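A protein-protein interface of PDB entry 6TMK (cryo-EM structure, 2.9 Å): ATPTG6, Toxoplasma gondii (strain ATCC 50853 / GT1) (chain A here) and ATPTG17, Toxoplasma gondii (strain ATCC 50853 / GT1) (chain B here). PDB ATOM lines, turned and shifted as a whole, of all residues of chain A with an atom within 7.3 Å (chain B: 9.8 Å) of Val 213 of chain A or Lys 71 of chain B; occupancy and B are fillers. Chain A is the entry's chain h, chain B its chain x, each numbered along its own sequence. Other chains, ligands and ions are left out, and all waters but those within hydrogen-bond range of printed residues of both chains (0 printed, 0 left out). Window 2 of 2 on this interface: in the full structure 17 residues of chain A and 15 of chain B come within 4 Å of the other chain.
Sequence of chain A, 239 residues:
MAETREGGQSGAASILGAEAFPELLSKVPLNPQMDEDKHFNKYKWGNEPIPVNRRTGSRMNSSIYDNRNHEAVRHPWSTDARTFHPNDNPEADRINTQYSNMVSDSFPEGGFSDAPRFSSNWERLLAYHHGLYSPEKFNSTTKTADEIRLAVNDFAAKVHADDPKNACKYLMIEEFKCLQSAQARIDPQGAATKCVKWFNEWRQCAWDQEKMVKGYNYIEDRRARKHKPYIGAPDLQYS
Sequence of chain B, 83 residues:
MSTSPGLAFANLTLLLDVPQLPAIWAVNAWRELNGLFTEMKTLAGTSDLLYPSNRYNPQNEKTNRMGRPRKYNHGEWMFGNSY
Of chain B, only Asn 64, Arg 68 and Lys 71 come within 4 Å of Val 213 of chain A.
Of the printed residues of chain B, Gly 215 of chain A touches Asn 64.
Glu 61 of chain B touches none of the printed residues of chain A.
Of the printed residues of chain A, Asn 64 of chain B touches Met 212, Val 213 and Gly 215.
Of chain A, only Val 213 comes within 4 Å of Lys 71 of chain B.
The nearest residue of chain B that does not touch Val 213 of chain A is Pro 69 of chain B (4.5 Å).
The nearest residue of chain A that does not touch Lys 71 of chain B is Lys 214 of chain A (5.1 Å).
The nearest printed residue of chain B that does not touch Tyr 216 of chain A is Arg 65 of chain B (5.4 Å).
Lys 211 of chain A touches Met 66 of chain B.
Met 212 of chain A touches Asn 64 of chain B.
Met 66 of chain B touches Met 212 of chain A (O to CE, 3.6 Å).
Met 212 of chain A touches Arg 68 of chain B (O to CG, 3.3 Å).
Val 213 of chain A touches Arg 68 of chain B.
CD of Lys 71 of chain B touches CG1 of Val 213 of chain A (3.7 Å).
The backbone NH (N) of Tyr 216 of chain A is in hydrogen-bond range of the backbone carbonyl oxygen (O) of Lys 211 of chain A (3.4 Å).
NZ of Lys 211 of chain A lies within salt-bridge range of OD1 of Asp 208 of chain A, at 2.6 Å.
The side-chain sulfur of Met 66 of chain B sits close to the backbone carbonyl oxygen of Tyr 216 of chain A (3.8 Å).
The backbone carbonyl oxygen of Val 213 of chain A sits at hydrogen-bond distance from the side-chain amide nitrogen of Asn 64 of chain B (2.6 Å).
The backbone NH (N) of Gly 215 of chain A lies close to the side-chain amide nitrogen (ND2) of Asn 64 of chain B, 3.2 Å away.
Hydrophobic or aromatic side chains of chain A that line the printed part of chain B: Met 212 and Val 213.
Hydrophobic or aromatic side chains of chain B within 4 Å of the printed part of chain A: Met 66.
Along chain B the printed residues that touch a printed residue of chain A span positions 64 to 71.
Among the printed residues, no Asp or Glu carboxylate lies within 4 Å of a Lys or Arg side-chain nitrogen of the other chain.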
ATOM      1  N   TRP A 207     -12.184   2.686   1.401  1.00  0.00           N
ATOM      2  CA  TRP A 207     -13.582   2.789   1.018  1.00  0.00           C
ATOM      3  C   TRP A 207     -14.334   1.492   1.269  1.00  0.00           C
ATOM      4  O   TRP A 207     -15.501   1.520   1.666  1.00  0.00           O
ATOM      5  CB  TRP A 207     -13.678   3.190  -0.450  1.00  0.00           C
ATOM      6  CG  TRP A 207     -15.014   2.950  -1.051  1.00  0.00           C
ATOM      7  CD1 TRP A 207     -15.314   2.054  -2.024  1.00  0.00           C
ATOM      8  CD2 TRP A 207     -16.240   3.597  -0.715  1.00  0.00           C
ATOM      9  NE1 TRP A 207     -16.644   2.101  -2.318  1.00  0.00           N
ATOM     10  CE2 TRP A 207     -17.237   3.043  -1.526  1.00  0.00           C
ATOM     11  CE3 TRP A 207     -16.591   4.589   0.194  1.00  0.00           C
ATOM     12  CZ2 TRP A 207     -18.554   3.451  -1.461  1.00  0.00           C
ATOM     13  CZ3 TRP A 207     -17.897   4.990   0.251  1.00  0.00           C
ATOM     14  CH2 TRP A 207     -18.861   4.423  -0.566  1.00  0.00           C
ATOM     15  N   ASP A 208     -13.704   0.345   1.017  1.00  0.00           N
ATOM     16  CA  ASP A 208     -14.393  -0.914   1.271  1.00  0.00           C
ATOM     17  C   ASP A 208     -14.743  -1.078   2.746  1.00  0.00           C
ATOM     18  O   ASP A 208     -15.854  -1.523   3.088  1.00  0.00           O
ATOM     19  CB  ASP A 208     -13.516  -2.068   0.795  1.00  0.00           C
ATOM     20  CG  ASP A 208     -13.295  -2.053  -0.701  1.00  0.00           C
ATOM     21  OD1 ASP A 208     -14.090  -1.414  -1.416  1.00  0.00           O
ATOM     22  OD2 ASP A 208     -12.316  -2.676  -1.160  1.00  0.00           O
ATOM     23  N   GLN A 209     -13.902  -0.539   3.624  1.00  0.00           N
ATOM     24  CA  GLN A 209     -14.193  -0.588   5.047  1.00  0.00           C
ATOM     25  C   GLN A 209     -15.250   0.433   5.418  1.00  0.00           C
ATOM     26  O   GLN A 209     -16.121   0.146   6.242  1.00  0.00           O
ATOM     27  CB  GLN A 209     -12.909  -0.369   5.843  1.00  0.00           C
ATOM     28  CG  GLN A 209     -12.961  -0.839   7.279  1.00  0.00           C
ATOM     29  CD  GLN A 209     -11.686  -0.564   8.053  1.00  0.00           C
ATOM     30  OE1 GLN A 209     -11.545  -1.001   9.195  1.00  0.00           O
ATOM     31  NE2 GLN A 209     -10.745   0.142   7.438  1.00  0.00           N
ATOM     32  N   GLU A 210     -15.170   1.641   4.864  1.00  0.00           N
ATOM     33  CA  GLU A 210     -16.179   2.632   5.202  1.00  0.00           C
ATOM     34  C   GLU A 210     -17.553   2.151   4.770  1.00  0.00           C
ATOM     35  O   GLU A 210     -18.538   2.351   5.484  1.00  0.00           O
ATOM     36  CB  GLU A 210     -15.855   3.967   4.548  1.00  0.00           C
ATOM     37  CG  GLU A 210     -16.635   5.123   5.115  1.00  0.00           C
ATOM     38  CD  GLU A 210     -16.071   5.618   6.431  1.00  0.00           C
ATOM     39  OE1 GLU A 210     -15.219   4.916   7.013  1.00  0.00           O
ATOM     40  OE2 GLU A 210     -16.482   6.706   6.886  1.00  0.00           O
ATOM     41  N   LYS A 211     -17.646   1.540   3.588  1.00  0.00           N
ATOM     42  CA  LYS A 211     -18.936   1.086   3.098  1.00  0.00           C
ATOM     43  C   LYS A 211     -19.424  -0.152   3.831  1.00  0.00           C
ATOM     44  O   LYS A 211     -20.624  -0.435   3.806  1.00  0.00           O
ATOM     45  CB  LYS A 211     -18.888   0.799   1.605  1.00  0.00           C
ATOM     46  CG  LYS A 211     -18.070  -0.386   1.223  1.00  0.00           C
ATOM     47  CD  LYS A 211     -18.164  -0.635  -0.239  1.00  0.00           C
ATOM     48  CE  LYS A 211     -17.439  -1.883  -0.643  1.00  0.00           C
ATOM     49  NZ  LYS A 211     -16.665  -1.723  -1.894  1.00  0.00           N
ATOM     50  N   MET A 212     -18.529  -0.896   4.487  1.00  0.00           N
ATOM     51  CA  MET A 212     -19.008  -2.001   5.309  1.00  0.00           C
ATOM     52  C   MET A 212     -19.455  -1.506   6.677  1.00  0.00           C
ATOM     53  O   MET A 212     -20.434  -2.009   7.235  1.00  0.00           O
ATOM     54  CB  MET A 212     -17.920  -3.063   5.455  1.00  0.00           C
ATOM     55  CG  MET A 212     -17.782  -3.974   4.265  1.00  0.00           C
ATOM     56  SD  MET A 212     -17.081  -5.575   4.674  1.00  0.00           S
ATOM     57  CE  MET A 212     -18.520  -6.381   5.355  1.00  0.00           C
ATOM     58  N   VAL A 213     -18.749  -0.520   7.226  1.00  0.00           N
ATOM     59  CA  VAL A 213     -19.128   0.065   8.507  1.00  0.00           C
ATOM     60  C   VAL A 213     -20.448   0.810   8.374  1.00  0.00           C
ATOM     61  O   VAL A 213     -21.434   0.496   9.048  1.00  0.00           O
ATOM     62  CB  VAL A 213     -18.008   0.982   9.025  1.00  0.00           C
ATOM     63  CG1 VAL A 213     -18.481   1.790  10.196  1.00  0.00           C
ATOM     64  CG2 VAL A 213     -16.804   0.161   9.402  1.00  0.00           C
ATOM     65  N   LYS A 214     -20.475   1.828   7.520  1.00  0.00           N
ATOM     66  CA  LYS A 214     -21.707   2.496   7.130  1.00  0.00           C
ATOM     67  C   LYS A 214     -22.319   1.704   5.989  1.00  0.00           C
ATOM     68  O   LYS A 214     -21.756   1.648   4.892  1.00  0.00           O
ATOM     69  CB  LYS A 214     -21.418   3.928   6.699  1.00  0.00           C
ATOM     70  CG  LYS A 214     -20.953   4.834   7.801  1.00  0.00           C
ATOM     71  CD  LYS A 214     -20.097   5.948   7.259  1.00  0.00           C
ATOM     72  CE  LYS A 214     -20.234   7.204   8.084  1.00  0.00           C
ATOM     73  NZ  LYS A 214     -21.478   7.943   7.739  1.00  0.00           N
ATOM     74  N   GLY A 215     -23.466   1.092   6.236  1.00  0.00           N
ATOM     75  CA  GLY A 215     -24.045   0.213   5.248  1.00  0.00           C
ATOM     76  C   GLY A 215     -24.452   0.935   3.988  1.00  0.00           C
ATOM     77  O   GLY A 215     -25.481   1.615   3.948  1.00  0.00           O
ATOM     78  N   TYR A 216     -23.654   0.774   2.941  1.00  0.00           N
ATOM     79  CA  TYR A 216     -23.910   1.395   1.652  1.00  0.00           C
ATOM     80  C   TYR A 216     -24.057   0.281   0.633  1.00  0.00           C
ATOM     81  O   TYR A 216     -23.165  -0.559   0.493  1.00  0.00           O
ATOM     82  CB  TYR A 216     -22.787   2.347   1.240  1.00  0.00           C
ATOM     83  CG  TYR A 216     -22.677   3.615   2.043  1.00  0.00           C
ATOM     84  CD1 TYR A 216     -23.788   4.201   2.615  1.00  0.00           C
ATOM     85  CD2 TYR A 216     -21.458   4.241   2.207  1.00  0.00           C
ATOM     86  CE1 TYR A 216     -23.683   5.359   3.340  1.00  0.00           C
ATOM     87  CE2 TYR A 216     -21.344   5.396   2.924  1.00  0.00           C
ATOM     88  CZ  TYR A 216     -22.458   5.954   3.488  1.00  0.00           C
ATOM     89  OH  TYR A 216     -22.335   7.115   4.209  1.00  0.00           O
ATOM     90  N   ASN B  60     -31.536  -5.683   9.303  1.00  0.00           N
ATOM     91  CA  ASN B  60     -32.632  -5.725  10.259  1.00  0.00           C
ATOM     92  C   ASN B  60     -32.458  -4.536  11.197  1.00  0.00           C
ATOM     93  O   ASN B  60     -31.743  -3.581  10.879  1.00  0.00           O
ATOM     94  CB  ASN B  60     -32.668  -7.072  10.997  1.00  0.00           C
ATOM     95  CG  ASN B  60     -31.498  -7.264  11.926  1.00  0.00           C
ATOM     96  OD1 ASN B  60     -31.372  -6.572  12.936  1.00  0.00           O
ATOM     97  ND2 ASN B  60     -30.648  -8.222  11.610  1.00  0.00           N
ATOM     98  N   GLU B  61     -33.125  -4.580  12.349  1.00  0.00           N
ATOM     99  CA  GLU B  61     -33.055  -3.462  13.279  1.00  0.00           C
ATOM    100  C   GLU B  61     -31.658  -3.294  13.860  1.00  0.00           C
ATOM    101  O   GLU B  61     -31.264  -2.175  14.208  1.00  0.00           O
ATOM    102  CB  GLU B  61     -34.070  -3.654  14.401  1.00  0.00           C
ATOM    103  CG  GLU B  61     -35.508  -3.508  13.958  1.00  0.00           C
ATOM    104  CD  GLU B  61     -36.070  -4.786  13.373  1.00  0.00           C
ATOM    105  OE1 GLU B  61     -35.273  -5.671  13.002  1.00  0.00           O
ATOM    106  OE2 GLU B  61     -37.309  -4.905  13.284  1.00  0.00           O
ATOM    107  N   LYS B  62     -30.900  -4.382  13.970  1.00  0.00           N
ATOM    108  CA  LYS B  62     -29.593  -4.376  14.611  1.00  0.00           C
ATOM    109  C   LYS B  62     -28.455  -4.639  13.635  1.00  0.00           C
ATOM    110  O   LYS B  62     -27.314  -4.827  14.068  1.00  0.00           O
ATOM    111  CB  LYS B  62     -29.559  -5.413  15.736  1.00  0.00           C
ATOM    112  CG  LYS B  62     -30.531  -5.152  16.874  1.00  0.00           C
ATOM    113  CD  LYS B  62     -30.009  -4.089  17.826  1.00  0.00           C
ATOM    114  CE  LYS B  62     -31.131  -3.399  18.585  1.00  0.00           C
ATOM    115  NZ  LYS B  62     -30.772  -2.004  18.971  1.00  0.00           N
ATOM    116  N   THR B  63     -28.728  -4.648  12.334  1.00  0.00           N
ATOM    117  CA  THR B  63     -27.748  -5.077  11.349  1.00  0.00           C
ATOM    118  C   THR B  63     -27.821  -4.196  10.112  1.00  0.00           C
ATOM    119  O   THR B  63     -28.909  -3.875   9.629  1.00  0.00           O
ATOM    120  CB  THR B  63     -27.972  -6.538  10.964  1.00  0.00           C
ATOM    121  OG1 THR B  63     -28.071  -7.333  12.150  1.00  0.00           O
ATOM    122  CG2 THR B  63     -26.851  -7.052  10.113  1.00  0.00           C
ATOM    123  N   ASN B  64     -26.650  -3.823   9.603  1.00  0.00           N
ATOM    124  CA  ASN B  64     -26.547  -3.019   8.399  1.00  0.00           C
ATOM    125  C   ASN B  64     -26.931  -3.831   7.166  1.00  0.00           C
ATOM    126  O   ASN B  64     -27.171  -5.038   7.223  1.00  0.00           O
ATOM    127  CB  ASN B  64     -25.126  -2.474   8.241  1.00  0.00           C
ATOM    128  CG  ASN B  64     -24.964  -1.098   8.818  1.00  0.00           C
ATOM    129  OD1 ASN B  64     -25.939  -0.421   9.138  1.00  0.00           O
ATOM    130  ND2 ASN B  64     -23.725  -0.669   8.948  1.00  0.00           N
ATOM    131  N   ARG B  65     -26.968  -3.142   6.032  1.00  0.00           N
ATOM    132  CA  ARG B  65     -27.151  -3.776   4.737  1.00  0.00           C
ATOM    133  C   ARG B  65     -25.889  -4.442   4.216  1.00  0.00           C
ATOM    134  O   ARG B  65     -25.867  -4.870   3.060  1.00  0.00           O
ATOM    135  CB  ARG B  65     -27.647  -2.747   3.727  1.00  0.00           C
ATOM    136  CG  ARG B  65     -28.991  -2.190   4.072  1.00  0.00           C
ATOM    137  CD  ARG B  65     -29.443  -1.132   3.111  1.00  0.00           C
ATOM    138  NE  ARG B  65     -30.615  -0.428   3.613  1.00  0.00           N
ATOM    139  CZ  ARG B  65     -31.168   0.621   3.020  1.00  0.00           C
ATOM    140  NH1 ARG B  65     -30.661   1.091   1.897  1.00  0.00           N
ATOM    141  NH2 ARG B  65     -32.229   1.199   3.553  1.00  0.00           N
ATOM    142  N   MET B  66     -24.839  -4.536   5.034  1.00  0.00           N
ATOM    143  CA  MET B  66     -23.646  -5.291   4.675  1.00  0.00           C
ATOM    144  C   MET B  66     -23.245  -6.259   5.779  1.00  0.00           C
ATOM    145  O   MET B  66     -22.116  -6.755   5.781  1.00  0.00           O
ATOM    146  CB  MET B  66     -22.483  -4.356   4.355  1.00  0.00           C
ATOM    147  CG  MET B  66     -22.763  -3.367   3.250  1.00  0.00           C
ATOM    148  SD  MET B  66     -23.182  -4.138   1.679  1.00  0.00           S
ATOM    149  CE  MET B  66     -21.609  -4.836   1.219  1.00  0.00           C
ATOM    150  N   GLY B  67     -24.145  -6.535   6.717  1.00  0.00           N
ATOM    151  CA  GLY B  67     -23.936  -7.546   7.721  1.00  0.00           C
ATOM    152  C   GLY B  67     -23.268  -7.072   8.987  1.00  0.00           C
ATOM    153  O   GLY B  67     -23.042  -7.886   9.889  1.00  0.00           O
ATOM    154  N   ARG B  68     -22.946  -5.804   9.085  1.00  0.00           N
ATOM    155  CA  ARG B  68     -22.313  -5.274  10.276  1.00  0.00           C
ATOM    156  C   ARG B  68     -23.361  -4.687  11.205  1.00  0.00           C
ATOM    157  O   ARG B  68     -24.495  -4.427  10.794  1.00  0.00           O
ATOM    158  CB  ARG B  68     -21.296  -4.195   9.896  1.00  0.00           C
ATOM    159  CG  ARG B  68     -20.123  -4.693   9.098  1.00  0.00           C
ATOM    160  CD  ARG B  68     -19.109  -5.395   9.954  1.00  0.00           C
ATOM    161  NE  ARG B  68     -17.813  -5.476   9.290  1.00  0.00           N
ATOM    162  CZ  ARG B  68     -16.938  -4.481   9.228  1.00  0.00           C
ATOM    163  NH1 ARG B  68     -17.206  -3.317   9.793  1.00  0.00           N
ATOM    164  NH2 ARG B  68     -15.788  -4.655   8.602  1.00  0.00           N
ATOM    165  N   PRO B  69     -23.023  -4.468  12.471  1.00  0.00           N
ATOM    166  CA  PRO B  69     -23.968  -3.805  13.370  1.00  0.00           C
ATOM    167  C   PRO B  69     -24.189  -2.351  12.995  1.00  0.00           C
ATOM    168  O   PRO B  69     -23.291  -1.664  12.504  1.00  0.00           O
ATOM    169  CB  PRO B  69     -23.299  -3.929  14.741  1.00  0.00           C
ATOM    170  CG  PRO B  69     -22.354  -5.055  14.593  1.00  0.00           C
ATOM    171  CD  PRO B  69     -21.852  -4.965  13.203  1.00  0.00           C
ATOM    172  N   ARG B  70     -25.406  -1.884  13.240  1.00  0.00           N
ATOM    173  CA  ARG B  70     -25.750  -0.507  12.926  1.00  0.00           C
ATOM    174  C   ARG B  70     -25.090   0.445  13.911  1.00  0.00           C
ATOM    175  O   ARG B  70     -25.104   0.213  15.124  1.00  0.00           O
ATOM    176  CB  ARG B  70     -27.261  -0.324  12.949  1.00  0.00           C
ATOM    177  CG  ARG B  70     -27.950  -0.753  11.690  1.00  0.00           C
ATOM    178  CD  ARG B  70     -29.429  -0.490  11.758  1.00  0.00           C
ATOM    179  NE  ARG B  70     -30.176  -1.257  10.771  1.00  0.00           N
ATOM    180  CZ  ARG B  70     -30.250  -0.949   9.484  1.00  0.00           C
ATOM    181  NH1 ARG B  70     -29.624   0.110   9.009  1.00  0.00           N
ATOM    182  NH2 ARG B  70     -30.954  -1.705   8.667  1.00  0.00           N
ATOM    183  N   LYS B  71     -24.508   1.515  13.385  1.00  0.00           N
ATOM    184  CA  LYS B  71     -23.935   2.558  14.219  1.00  0.00           C
ATOM    185  C   LYS B  71     -25.022   3.484  14.745  1.00  0.00           C
ATOM    186  O   LYS B  71     -25.975   3.813  14.035  1.00  0.00           O
ATOM    187  CB  LYS B  71     -22.899   3.362  13.439  1.00  0.00           C
ATOM    188  CG  LYS B  71     -21.556   2.686  13.331  1.00  0.00           C
ATOM    189  CD  LYS B  71     -20.517   3.617  12.756  1.00  0.00           C
ATOM    190  CE  LYS B  71     -19.806   4.369  13.853  1.00  0.00           C
ATOM    191  NZ  LYS B  71     -18.909   3.486  14.641  1.00  0.00           N
ATOM    192  N   TYR B  72     -24.872   3.907  15.999  1.00  0.00           N
ATOM    193  CA  TYR B  72     -25.786   4.870  16.609  1.00  0.00           C
ATOM    194  C   TYR B  72     -27.203   4.314  16.696  1.00  0.00           C
ATOM    195  O   TYR B  72     -28.180   5.007  16.410  1.00  0.00           O
ATOM    196  CB  TYR B  72     -25.770   6.186  15.835  1.00  0.00           C
ATOM    197  CG  TYR B  72     -24.387   6.643  15.458  1.00  0.00           C
ATOM    198  CD1 TYR B  72     -23.369   6.671  16.391  1.00  0.00           C
ATOM    199  CD2 TYR B  72     -24.099   7.042  14.168  1.00  0.00           C
ATOM    200  CE1 TYR B  72     -22.104   7.082  16.048  1.00  0.00           C
ATOM    201  CE2 TYR B  72     -22.840   7.455  13.817  1.00  0.00           C
ATOM    202  CZ  TYR B  72     -21.846   7.475  14.762  1.00  0.00           C
ATOM    203  OH  TYR B  72     -20.579   7.885  14.426  1.00  0.00           O
ATOM    204  N   ASN B  73     -27.315   3.050  17.099  1.00  0.00           N
ATOM    205  CA  ASN B  73     -28.594   2.355  17.168  1.00  0.00           C
ATOM    206  C   ASN B  73     -28.963   1.946  18.588  1.00  0.00           C
ATOM    207  O   ASN B  73     -29.892   1.153  18.769  1.00  0.00           O
ATOM    208  CB  ASN B  73     -28.570   1.125  16.262  1.00  0.00           C
ATOM    209  CG  ASN B  73     -29.938   0.756  15.746  1.00  0.00           C
ATOM    210  OD1 ASN B  73     -30.699   1.613  15.302  1.00  0.00           O
ATOM    211  ND2 ASN B  73     -30.260  -0.526  15.802  1.00  0.00           N
ATOM    212  N   HIS B  74     -28.270   2.469  19.599  1.00  0.00           N
ATOM    213  CA  HIS B  74     -28.537   2.068  20.975  1.00  0.00           C
ATOM    214  C   HIS B  74     -29.759   2.779  21.539  1.00  0.00           C
ATOM    215  O   HIS B  74     -30.534   2.180  22.293  1.00  0.00           O
ATOM    216  CB  HIS B  74     -27.313   2.353  21.843  1.00  0.00           C
ATOM    217  CG  HIS B  74     -27.477   1.947  23.273  1.00  0.00           C
ATOM    218  ND1 HIS B  74     -28.057   2.765  24.217  1.00  0.00           N
ATOM    219  CD2 HIS B  74     -27.120   0.815  23.925  1.00  0.00           C
ATOM    220  CE1 HIS B  74     -28.061   2.150  25.387  1.00  0.00           C
ATOM    221  NE2 HIS B  74     -27.499   0.965  25.236  1.00  0.00           N
ATOM    222  N   GLY B  75     -29.950   4.049  21.188  1.00  0.00           N
ATOM    223  CA  GLY B  75     -31.061   4.829  21.682  1.00  0.00           C
ATOM    224  C   GLY B  75     -32.230   4.843  20.715  1.00  0.00           C
ATOM    225  O   GLY B  75     -32.251   4.150  19.696  1.00  0.00           O
ATOM    226  N   ASN B  81     -37.325   5.010  12.986  1.00  0.00           N
ATOM    227  CA  ASN B  81     -36.153   4.280  12.532  1.00  0.00           C
ATOM    228  C   ASN B  81     -35.130   5.234  11.936  1.00  0.00           C
ATOM    229  O   ASN B  81     -35.469   6.271  11.363  1.00  0.00           O
ATOM    230  CB  ASN B  81     -36.546   3.227  11.504  1.00  0.00           C
ATOM    231  CG  ASN B  81     -37.218   2.031  12.128  1.00  0.00           C
ATOM    232  OD1 ASN B  81     -36.915   1.657  13.261  1.00  0.00           O
ATOM    233  ND2 ASN B  81     -38.132   1.414  11.391  1.00  0.00           N
ATOM    234  N   SER B  82     -33.864   4.863  12.066  1.00  0.00           N
ATOM    235  CA  SER B  82     -32.766   5.663  11.556  1.00  0.00           C
ATOM    236  C   SER B  82     -32.486   5.404  10.089  1.00  0.00           C
ATOM    237  O   SER B  82     -31.381   5.685   9.617  1.00  0.00           O
ATOM    238  CB  SER B  82     -31.516   5.380  12.381  1.00  0.00           C
ATOM    239  OG  SER B  82     -31.805   5.446  13.763  1.00  0.00           O
ATOM    240  N   TYR B  83     -33.464   4.877   9.364  1.00  0.00           N
ATOM    241  CA  TYR B  83     -33.256   4.429   7.999  1.00  0.00           C
ATOM    242  C   TYR B  83     -34.570   4.376   7.232  1.00  0.00           C
ATOM    243  O   TYR B  83     -35.610   4.786   7.740  1.00  0.00           O
ATOM    244  CB  TYR B  83     -32.564   3.065   7.984  1.00  0.00           C
ATOM    245  CG  TYR B  83     -33.112   2.063   8.969  1.00  0.00           C
ATOM    246  CD1 TYR B  83     -32.452   1.808  10.156  1.00  0.00           C
ATOM    247  CD2 TYR B  83     -34.272   1.365   8.708  1.00  0.00           C
ATOM    248  CE1 TYR B  83     -32.938   0.897  11.057  1.00  0.00           C
ATOM    249  CE2 TYR B  83     -34.764   0.450   9.605  1.00  0.00           C
ATOM    250  CZ  TYR B  83     -34.094   0.219  10.778  1.00  0.00           C
ATOM    251  OH  TYR B  83     -34.583  -0.696  11.677  1.00  0.00           O
